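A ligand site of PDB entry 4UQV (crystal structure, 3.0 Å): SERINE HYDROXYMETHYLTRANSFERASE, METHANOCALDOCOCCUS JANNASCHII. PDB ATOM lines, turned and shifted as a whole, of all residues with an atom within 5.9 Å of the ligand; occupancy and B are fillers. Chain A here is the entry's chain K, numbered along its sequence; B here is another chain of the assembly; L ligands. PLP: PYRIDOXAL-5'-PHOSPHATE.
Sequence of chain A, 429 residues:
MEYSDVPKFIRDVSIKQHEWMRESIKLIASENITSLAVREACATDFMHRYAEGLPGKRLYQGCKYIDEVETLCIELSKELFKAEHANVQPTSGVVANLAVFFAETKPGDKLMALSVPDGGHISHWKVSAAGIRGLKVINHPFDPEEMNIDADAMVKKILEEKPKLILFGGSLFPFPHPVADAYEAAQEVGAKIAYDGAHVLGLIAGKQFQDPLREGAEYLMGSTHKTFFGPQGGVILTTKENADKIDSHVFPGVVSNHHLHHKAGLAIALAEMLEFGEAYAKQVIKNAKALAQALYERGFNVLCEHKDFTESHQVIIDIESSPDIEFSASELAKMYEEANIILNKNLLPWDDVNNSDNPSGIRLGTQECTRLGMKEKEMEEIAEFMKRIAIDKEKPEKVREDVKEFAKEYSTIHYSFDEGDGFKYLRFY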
ATOM      1  N   SER A  30      -7.089 -14.263 -18.132  1.00  0.00           N
ATOM      2  CA  SER A  30      -6.351 -13.235 -17.408  1.00  0.00           C
ATOM      3  C   SER A  30      -4.829 -13.442 -17.312  1.00  0.00           C
ATOM      4  O   SER A  30      -4.139 -12.654 -16.680  1.00  0.00           O
ATOM      5  CB  SER A  30      -6.920 -13.105 -15.992  1.00  0.00           C
ATOM      6  OG  SER A  30      -8.300 -12.789 -16.039  1.00  0.00           O
ATOM      7  N   SER A  92      -1.743  -2.202  -8.664  1.00  0.00           N
ATOM      8  CA  SER A  92      -2.524  -3.257  -9.308  1.00  0.00           C
ATOM      9  C   SER A  92      -3.710  -2.638 -10.044  1.00  0.00           C
ATOM     10  O   SER A  92      -3.893  -1.411 -10.019  1.00  0.00           O
ATOM     11  CB  SER A  92      -3.012  -4.272  -8.285  1.00  0.00           C
ATOM     12  OG  SER A  92      -3.792  -3.656  -7.276  1.00  0.00           O
ATOM     13  N   GLY A  93      -4.517  -3.469 -10.690  1.00  0.00           N
ATOM     14  CA  GLY A  93      -5.673  -2.991 -11.422  1.00  0.00           C
ATOM     15  C   GLY A  93      -6.763  -2.497 -10.501  1.00  0.00           C
ATOM     16  O   GLY A  93      -7.395  -1.462 -10.745  1.00  0.00           O
ATOM     17  N   VAL A  94      -6.995  -3.241  -9.421  1.00  0.00           N
ATOM     18  CA  VAL A  94      -8.043  -2.901  -8.467  1.00  0.00           C
ATOM     19  C   VAL A  94      -7.737  -1.574  -7.778  1.00  0.00           C
ATOM     20  O   VAL A  94      -8.638  -0.787  -7.474  1.00  0.00           O
ATOM     21  CB  VAL A  94      -8.220  -4.023  -7.408  1.00  0.00           C
ATOM     22  CG1 VAL A  94      -6.882  -4.391  -6.785  1.00  0.00           C
ATOM     23  CG2 VAL A  94      -9.235  -3.621  -6.350  1.00  0.00           C
ATOM     24  N   VAL A  95      -6.451  -1.313  -7.553  1.00  0.00           N
ATOM     25  CA  VAL A  95      -6.032  -0.032  -6.985  1.00  0.00           C
ATOM     26  C   VAL A  95      -6.303   1.091  -7.973  1.00  0.00           C
ATOM     27  O   VAL A  95      -6.696   2.191  -7.584  1.00  0.00           O
ATOM     28  CB  VAL A  95      -4.542  -0.049  -6.605  1.00  0.00           C
ATOM     29  CG1 VAL A  95      -4.091   1.313  -6.133  1.00  0.00           C
ATOM     30  CG2 VAL A  95      -4.293  -1.092  -5.523  1.00  0.00           C
ATOM     31  N   ASN A  97      -8.733   1.070 -10.155  1.00  0.00           N
ATOM     32  CA  ASN A  97     -10.173   1.264 -10.018  1.00  0.00           C
ATOM     33  C   ASN A  97     -10.495   2.156  -8.827  1.00  0.00           C
ATOM     34  O   ASN A  97     -11.087   3.224  -8.997  1.00  0.00           O
ATOM     35  CB  ASN A  97     -10.898  -0.079  -9.865  1.00  0.00           C
ATOM     36  CG  ASN A  97     -10.855  -0.920 -11.131  1.00  0.00           C
ATOM     37  OD1 ASN A  97      -9.909  -0.843 -11.906  1.00  0.00           O
ATOM     38  ND2 ASN A  97     -11.886  -1.715 -11.339  1.00  0.00           N
ATOM     39  N   HIS A 121     -16.595  -8.294 -13.473  1.00  0.00           N
ATOM     40  CA  HIS A 121     -15.380  -8.756 -12.805  1.00  0.00           C
ATOM     41  C   HIS A 121     -15.530  -8.298 -11.369  1.00  0.00           C
ATOM     42  O   HIS A 121     -16.347  -7.428 -11.094  1.00  0.00           O
ATOM     43  CB  HIS A 121     -14.132  -8.163 -13.467  1.00  0.00           C
ATOM     44  CG  HIS A 121     -12.934  -8.114 -12.575  1.00  0.00           C
ATOM     45  ND1 HIS A 121     -12.198  -9.249 -12.257  1.00  0.00           N
ATOM     46  CD2 HIS A 121     -12.346  -7.094 -11.917  1.00  0.00           C
ATOM     47  CE1 HIS A 121     -11.212  -8.908 -11.450  1.00  0.00           C
ATOM     48  NE2 HIS A 121     -11.269  -7.612 -11.233  1.00  0.00           N
ATOM     49  N   ILE A 122     -14.766  -8.856 -10.423  1.00  0.00           N
ATOM     50  CA  ILE A 122     -15.009  -8.405  -9.075  1.00  0.00           C
ATOM     51  C   ILE A 122     -14.162  -7.174  -8.855  1.00  0.00           C
ATOM     52  O   ILE A 122     -12.985  -7.252  -8.494  1.00  0.00           O
ATOM     53  CB  ILE A 122     -14.656  -9.470  -8.025  1.00  0.00           C
ATOM     54  CG1 ILE A 122     -14.987 -10.874  -8.530  1.00  0.00           C
ATOM     55  CG2 ILE A 122     -15.334  -9.165  -6.699  1.00  0.00           C
ATOM     56  CD1 ILE A 122     -13.794 -11.628  -9.104  1.00  0.00           C
ATOM     57  N   SER A 123     -14.796  -6.027  -9.066  1.00  0.00           N
ATOM     58  CA  SER A 123     -14.304  -4.752  -8.617  1.00  0.00           C
ATOM     59  C   SER A 123     -15.469  -3.939  -8.094  1.00  0.00           C
ATOM     60  O   SER A 123     -15.672  -3.820  -6.902  1.00  0.00           O
ATOM     61  CB  SER A 123     -13.587  -4.015  -9.752  1.00  0.00           C
ATOM     62  OG  SER A 123     -14.392  -3.978 -10.916  1.00  0.00           O
ATOM     63  N   HIS A 124     -16.295  -3.474  -9.038  1.00  0.00           N
ATOM     64  CA  HIS A 124     -17.278  -2.421  -8.814  1.00  0.00           C
ATOM     65  C   HIS A 124     -18.326  -2.767  -7.759  1.00  0.00           C
ATOM     66  O   HIS A 124     -18.760  -1.920  -6.984  1.00  0.00           O
ATOM     67  CB  HIS A 124     -17.987  -2.091 -10.125  1.00  0.00           C
ATOM     68  CG  HIS A 124     -17.146  -2.328 -11.348  1.00  0.00           C
ATOM     69  ND1 HIS A 124     -16.058  -1.543 -11.661  1.00  0.00           N
ATOM     70  CD2 HIS A 124     -17.243  -3.254 -12.327  1.00  0.00           C
ATOM     71  CE1 HIS A 124     -15.519  -1.979 -12.789  1.00  0.00           C
ATOM     72  NE2 HIS A 124     -16.217  -3.018 -13.215  1.00  0.00           N
ATOM     73  N   GLY A 170     -14.920  -5.534 -18.938  1.00  0.00           N
ATOM     74  CA  GLY A 170     -15.264  -6.574 -17.990  1.00  0.00           C
ATOM     75  C   GLY A 170     -14.515  -7.883 -18.178  1.00  0.00           C
ATOM     76  O   GLY A 170     -13.552  -7.953 -18.946  1.00  0.00           O
ATOM     77  N   ASP A 196     -12.293   0.299 -18.208  1.00  0.00           N
ATOM     78  CA  ASP A 196     -11.235  -0.533 -17.668  1.00  0.00           C
ATOM     79  C   ASP A 196     -10.681  -1.319 -18.842  1.00  0.00           C
ATOM     80  O   ASP A 196     -11.351  -2.176 -19.405  1.00  0.00           O
ATOM     81  CB  ASP A 196     -11.748  -1.449 -16.562  1.00  0.00           C
ATOM     82  CG  ASP A 196     -10.654  -2.298 -15.957  1.00  0.00           C
ATOM     83  OD1 ASP A 196      -9.878  -1.775 -15.144  1.00  0.00           O
ATOM     84  OD2 ASP A 196     -10.581  -3.507 -16.296  1.00  0.00           O
ATOM     85  N   ALA A 198      -8.100  -3.297 -18.919  1.00  0.00           N
ATOM     86  CA  ALA A 198      -7.217  -4.381 -18.501  1.00  0.00           C
ATOM     87  C   ALA A 198      -7.283  -5.604 -19.407  1.00  0.00           C
ATOM     88  O   ALA A 198      -6.316  -5.925 -20.104  1.00  0.00           O
ATOM     89  CB  ALA A 198      -7.554  -4.787 -17.067  1.00  0.00           C
ATOM     90  N   HIS A 199      -8.444  -6.260 -19.418  1.00  0.00           N
ATOM     91  CA  HIS A 199      -8.620  -7.490 -20.188  1.00  0.00           C
ATOM     92  C   HIS A 199      -8.264  -7.313 -21.663  1.00  0.00           C
ATOM     93  O   HIS A 199      -7.667  -8.191 -22.273  1.00  0.00           O
ATOM     94  CB  HIS A 199     -10.063  -7.987 -20.061  1.00  0.00           C
ATOM     95  CG  HIS A 199     -10.193  -9.470 -19.972  1.00  0.00           C
ATOM     96  ND1 HIS A 199      -9.238 -10.331 -20.474  1.00  0.00           N
ATOM     97  CD2 HIS A 199     -11.150 -10.250 -19.424  1.00  0.00           C
ATOM     98  CE1 HIS A 199      -9.606 -11.580 -20.250  1.00  0.00           C
ATOM     99  NE2 HIS A 199     -10.762 -11.560 -19.618  1.00  0.00           N
ATOM    100  N   MET A 221      -8.236   2.893 -17.675  1.00  0.00           N
ATOM    101  CA  MET A 221      -7.276   2.367 -16.697  1.00  0.00           C
ATOM    102  C   MET A 221      -7.317   0.852 -16.625  1.00  0.00           C
ATOM    103  O   MET A 221      -8.267   0.234 -17.101  1.00  0.00           O
ATOM    104  CB  MET A 221      -7.540   2.974 -15.316  1.00  0.00           C
ATOM    105  CG  MET A 221      -8.887   3.669 -15.175  1.00  0.00           C
ATOM    106  SD  MET A 221     -10.282   2.566 -15.434  1.00  0.00           S
ATOM    107  CE  MET A 221      -9.961   1.347 -14.172  1.00  0.00           C
ATOM    108  N   GLY A 222      -6.279   0.241 -16.063  1.00  0.00           N
ATOM    109  CA  GLY A 222      -6.300  -1.199 -15.917  1.00  0.00           C
ATOM    110  C   GLY A 222      -4.995  -1.887 -15.558  1.00  0.00           C
ATOM    111  O   GLY A 222      -3.969  -1.245 -15.351  1.00  0.00           O
ATOM    112  N   SER A 223      -5.063  -3.217 -15.491  1.00  0.00           N
ATOM    113  CA  SER A 223      -3.919  -4.034 -15.114  1.00  0.00           C
ATOM    114  C   SER A 223      -2.955  -4.217 -16.273  1.00  0.00           C
ATOM    115  O   SER A 223      -3.374  -4.397 -17.422  1.00  0.00           O
ATOM    116  CB  SER A 223      -4.396  -5.401 -14.597  1.00  0.00           C
ATOM    117  OG  SER A 223      -4.978  -6.176 -15.638  1.00  0.00           O
ATOM    118  N   THR A 224      -1.671  -4.186 -15.965  1.00  0.00           N
ATOM    119  CA  THR A 224      -0.637  -4.305 -16.987  1.00  0.00           C
ATOM    120  C   THR A 224      -0.172  -5.742 -17.182  1.00  0.00           C
ATOM    121  O   THR A 224       0.626  -6.029 -18.066  1.00  0.00           O
ATOM    122  CB  THR A 224       0.591  -3.443 -16.631  1.00  0.00           C
ATOM    123  OG1 THR A 224       1.170  -3.894 -15.406  1.00  0.00           O
ATOM    124  CG2 THR A 224       0.188  -1.977 -16.494  1.00  0.00           C
ATOM    125  N   HIS A 225      -0.678  -6.662 -16.365  1.00  0.00           N
ATOM    126  CA  HIS A 225      -0.235  -8.049 -16.406  1.00  0.00           C
ATOM    127  C   HIS A 225      -1.129  -8.965 -17.246  1.00  0.00           C
ATOM    128  O   HIS A 225      -0.892 -10.175 -17.312  1.00  0.00           O
ATOM    129  CB  HIS A 225      -0.117  -8.610 -14.988  1.00  0.00           C
ATOM    130  CG  HIS A 225      -1.262  -8.238 -14.095  1.00  0.00           C
ATOM    131  ND1 HIS A 225      -1.187  -7.215 -13.178  1.00  0.00           N
ATOM    132  CD2 HIS A 225      -2.506  -8.750 -13.979  1.00  0.00           C
ATOM    133  CE1 HIS A 225      -2.330  -7.110 -12.532  1.00  0.00           C
ATOM    134  NE2 HIS A 225      -3.154  -8.033 -12.996  1.00  0.00           N
ATOM    135  N   LYS A 226      -2.151  -8.404 -17.871  1.00  0.00           N
ATOM    136  CA  LYS A 226      -3.058  -9.201 -18.671  1.00  0.00           C
ATOM    137  C   LYS A 226      -3.265  -8.563 -19.984  1.00  0.00           C
ATOM    138  O   LYS A 226      -3.538  -7.372 -20.054  1.00  0.00           O
ATOM    139  CB  LYS A 226      -4.339  -9.464 -17.897  1.00  0.00           C
ATOM    140  CG  LYS A 226      -5.686  -8.936 -18.421  1.00  0.00           C
ATOM    141  CD  LYS A 226      -6.943  -9.374 -17.670  1.00  0.00           C
ATOM    142  CE  LYS A 226      -6.993  -9.103 -16.171  1.00  0.00           C
ATOM    143  NZ  LYS A 226      -7.987  -8.137 -15.679  1.00  0.00           N
ATOM    144  N   GLN A 232       2.942  -7.352 -12.728  1.00  0.00           N
ATOM    145  CA  GLN A 232       1.763  -7.067 -11.916  1.00  0.00           C
ATOM    146  C   GLN A 232       1.731  -5.621 -11.450  1.00  0.00           C
ATOM    147  O   GLN A 232       2.659  -5.141 -10.792  1.00  0.00           O
ATOM    148  CB  GLN A 232       1.693  -8.010 -10.721  1.00  0.00           C
ATOM    149  CG  GLN A 232       1.520  -9.483 -11.099  1.00  0.00           C
ATOM    150  CD  GLN A 232       0.225 -10.064 -10.567  1.00  0.00           C
ATOM    151  OE1 GLN A 232       0.232 -11.052  -9.831  1.00  0.00           O
ATOM    152  NE2 GLN A 232      -0.890  -9.466 -10.956  1.00  0.00           N
ATOM    153  N   GLY A 233       0.651  -4.918 -11.790  1.00  0.00           N
ATOM    154  CA  GLY A 233       0.475  -3.533 -11.396  1.00  0.00           C
ATOM    155  C   GLY A 233      -0.594  -2.873 -12.241  1.00  0.00           C
ATOM    156  O   GLY A 233      -0.999  -3.413 -13.263  1.00  0.00           O
ATOM    157  N   TYR B  50      -3.028 -16.520 -10.599  1.00  0.00           N
ATOM    158  CA  TYR B  50      -4.083 -16.064  -9.703  1.00  0.00           C
ATOM    159  C   TYR B  50      -4.585 -17.194  -8.802  1.00  0.00           C
ATOM    160  O   TYR B  50      -4.877 -18.291  -9.282  1.00  0.00           O
ATOM    161  CB  TYR B  50      -5.246 -15.475 -10.503  1.00  0.00           C
ATOM    162  CG  TYR B  50      -5.043 -14.025 -10.887  1.00  0.00           C
ATOM    163  CD1 TYR B  50      -5.375 -13.002 -10.009  1.00  0.00           C
ATOM    164  CD2 TYR B  50      -4.500 -13.697 -12.121  1.00  0.00           C
ATOM    165  CE1 TYR B  50      -5.178 -11.683 -10.350  1.00  0.00           C
ATOM    166  CE2 TYR B  50      -4.300 -12.369 -12.465  1.00  0.00           C
ATOM    167  CZ  TYR B  50      -4.642 -11.371 -11.575  1.00  0.00           C
ATOM    168  OH  TYR B  50      -4.444 -10.056 -11.925  1.00  0.00           O
ATOM    169  N   VAL B 254      -9.376  -7.185  -2.830  1.00  0.00           N
ATOM    170  CA  VAL B 254      -8.272  -6.786  -3.687  1.00  0.00           C
ATOM    171  C   VAL B 254      -7.775  -7.995  -4.446  1.00  0.00           C
ATOM    172  O   VAL B 254      -7.286  -8.951  -3.852  1.00  0.00           O
ATOM    173  CB  VAL B 254      -7.130  -6.151  -2.881  1.00  0.00           C
ATOM    174  CG1 VAL B 254      -5.888  -6.020  -3.734  1.00  0.00           C
ATOM    175  CG2 VAL B 254      -7.558  -4.800  -2.328  1.00  0.00           C
ATOM    176  N   VAL B 255      -7.908  -7.937  -5.767  1.00  0.00           N
ATOM    177  CA  VAL B 255      -7.467  -9.042  -6.623  1.00  0.00           C
ATOM    178  C   VAL B 255      -6.228  -8.649  -7.408  1.00  0.00           C
ATOM    179  O   VAL B 255      -5.198  -9.334  -7.358  1.00  0.00           O
ATOM    180  CB  VAL B 255      -8.576  -9.467  -7.603  1.00  0.00           C
ATOM    181  CG1 VAL B 255      -9.014  -8.290  -8.453  1.00  0.00           C
ATOM    182  CG2 VAL B 255      -8.085 -10.620  -8.468  1.00  0.00           C
ATOM    183  N   HIS B 258      -4.315 -11.237  -6.346  1.00  0.00           N
ATOM    184  CA  HIS B 258      -3.137 -11.713  -5.615  1.00  0.00           C
ATOM    185  C   HIS B 258      -1.875 -11.541  -6.444  1.00  0.00           C
ATOM    186  O   HIS B 258      -1.905 -11.677  -7.665  1.00  0.00           O
ATOM    187  CB  HIS B 258      -3.315 -13.184  -5.231  1.00  0.00           C
ATOM    188  CG  HIS B 258      -2.475 -13.616  -4.067  1.00  0.00           C
ATOM    189  ND1 HIS B 258      -2.289 -14.937  -3.731  1.00  0.00           N
ATOM    190  CD2 HIS B 258      -1.784 -12.901  -3.152  1.00  0.00           C
ATOM    191  CE1 HIS B 258      -1.511 -15.015  -2.670  1.00  0.00           C
ATOM    192  NE2 HIS B 258      -1.193 -13.788  -2.289  1.00  0.00           N
ATOM    193  N   HIS B 259      -0.766 -11.230  -5.787  1.00  0.00           N
ATOM    194  CA  HIS B 259       0.525 -11.221  -6.466  1.00  0.00           C
ATOM    195  C   HIS B 259       1.375 -12.359  -5.898  1.00  0.00           C
ATOM    196  O   HIS B 259       1.872 -12.286  -4.784  1.00  0.00           O
ATOM    197  CB  HIS B 259       1.217  -9.871  -6.299  1.00  0.00           C
ATOM    198  CG  HIS B 259       0.439  -8.732  -6.855  1.00  0.00           C
ATOM    199  ND1 HIS B 259      -0.576  -8.892  -7.777  1.00  0.00           N
ATOM    200  CD2 HIS B 259       0.509  -7.396  -6.623  1.00  0.00           C
ATOM    201  CE1 HIS B 259      -1.087  -7.715  -8.090  1.00  0.00           C
ATOM    202  NE2 HIS B 259      -0.439  -6.785  -7.396  1.00  0.00           N
HETATM  203  N1  PLP L   1      -9.153  -5.218 -11.683  1.00  0.00           N
HETATM  204  C2  PLP L   1      -9.798  -5.314 -12.845  1.00  0.00           C
HETATM  205  C2A PLP L   1     -10.793  -4.262 -13.226  1.00  0.00           C
HETATM  206  C3  PLP L   1      -9.552  -6.368 -13.708  1.00  0.00           C
HETATM  207  O3  PLP L   1     -10.215  -6.439 -14.905  1.00  0.00           O
HETATM  208  C4  PLP L   1      -8.625  -7.351 -13.363  1.00  0.00           C
HETATM  209  C4A PLP L   1      -8.387  -8.489 -14.330  1.00  0.00           C
HETATM  210  C5  PLP L   1      -7.962  -7.225 -12.127  1.00  0.00           C
HETATM  211  C6  PLP L   1      -8.263  -6.134 -11.306  1.00  0.00           C
HETATM  212  C5A PLP L   1      -6.937  -8.228 -11.647  1.00  0.00           C
HETATM  213  O4P PLP L   1      -6.330  -8.018 -10.432  1.00  0.00           O
HETATM  214  P   PLP L   1      -5.187  -6.973 -10.349  1.00  0.00           P
HETATM  215  O1P PLP L   1      -3.908  -7.709 -10.056  1.00  0.00           O
HETATM  216  O2P PLP L   1      -5.099  -6.240 -11.661  1.00  0.00           O
HETATM  217  O3P PLP L   1      -5.497  -6.014  -9.225  1.00  0.00           O
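NZ of Lys 226 is bonded to C4A of the ligand (1.5 Å). O1P of the ligand lies within hydrogen-bond range of OH of Tyr 50 of chain B (3.0 Å). The side-chain carboxylate (OD2) of Asp 196 lies close to an oxygen (O3) of the ligand. A ring nitrogen (NE2) of His 225 is in hydrogen-bond range of an oxygen (O2P) of the ligand, at 3.0 Å. N of Val 94 sits at hydrogen-bond distance from O3P of the ligand (3.2 Å). The backbone NH (N) of Gly 93 lies within hydrogen-bond range of an oxygen (O2P) of the ligand, 3.0 Å away. NE2 of His 121 lies close to N1 of the ligand.
The side-chain amide oxygen (OD1) of Asn 97 lies close to the side-chain carboxylate (OD1) of Asp 196, 3.4 Å away. NE2 of His 225 sits at hydrogen-bond distance from OH of Tyr 50 of chain B. N of Gly 233 sits at hydrogen-bond distance from ND1 of His 225, at 3.3 Å. OE1 of Gln 232 lies close to O of His 258 of chain B, at 3.1 Å. The side-chain hydroxyl (OG) of Ser 123 sits close to the side-chain amide nitrogen (ND2) of Asn 97, at 3.4 Å. The side-chain amide oxygen of Asn 97 lies close to the backbone carbonyl oxygen of Gly 93, 2.8 Å away. A ring nitrogen (ND1) of His 259 of chain B lies within hydrogen-bond range of the side-chain amide oxygen (OE1) of Gln 232 (3.1 Å). A ring nitrogen (ND1) of His 225 is in hydrogen-bond range of the side-chain amide nitrogen (NE2) of Gln 232 (3.2 Å).
O of Val 255 of chain B sits close to O1P of the ligand, at 3.4 Å. Merely in contact with the ligand: Ser 92 (3.2 Å), Asn 97 (3.4 Å), Ala 198 (3.8 Å), Ser 223 (3.1 Å), Gln 232 (3.6 Å) and His 259 of chain B (3.4 Å). Hydrophobic or aromatic side chains within 4 Å of the ligand: Val 94, His 121, Ala 198, His 225, Tyr 50 of chain B, Val 255 of chain B and His 259 of chain B. Of the 27 residues printed, 14 come within 4 Å of the ligand. The nearest printed residue that does not touch the ligand is Ser 123 (4.3 Å).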
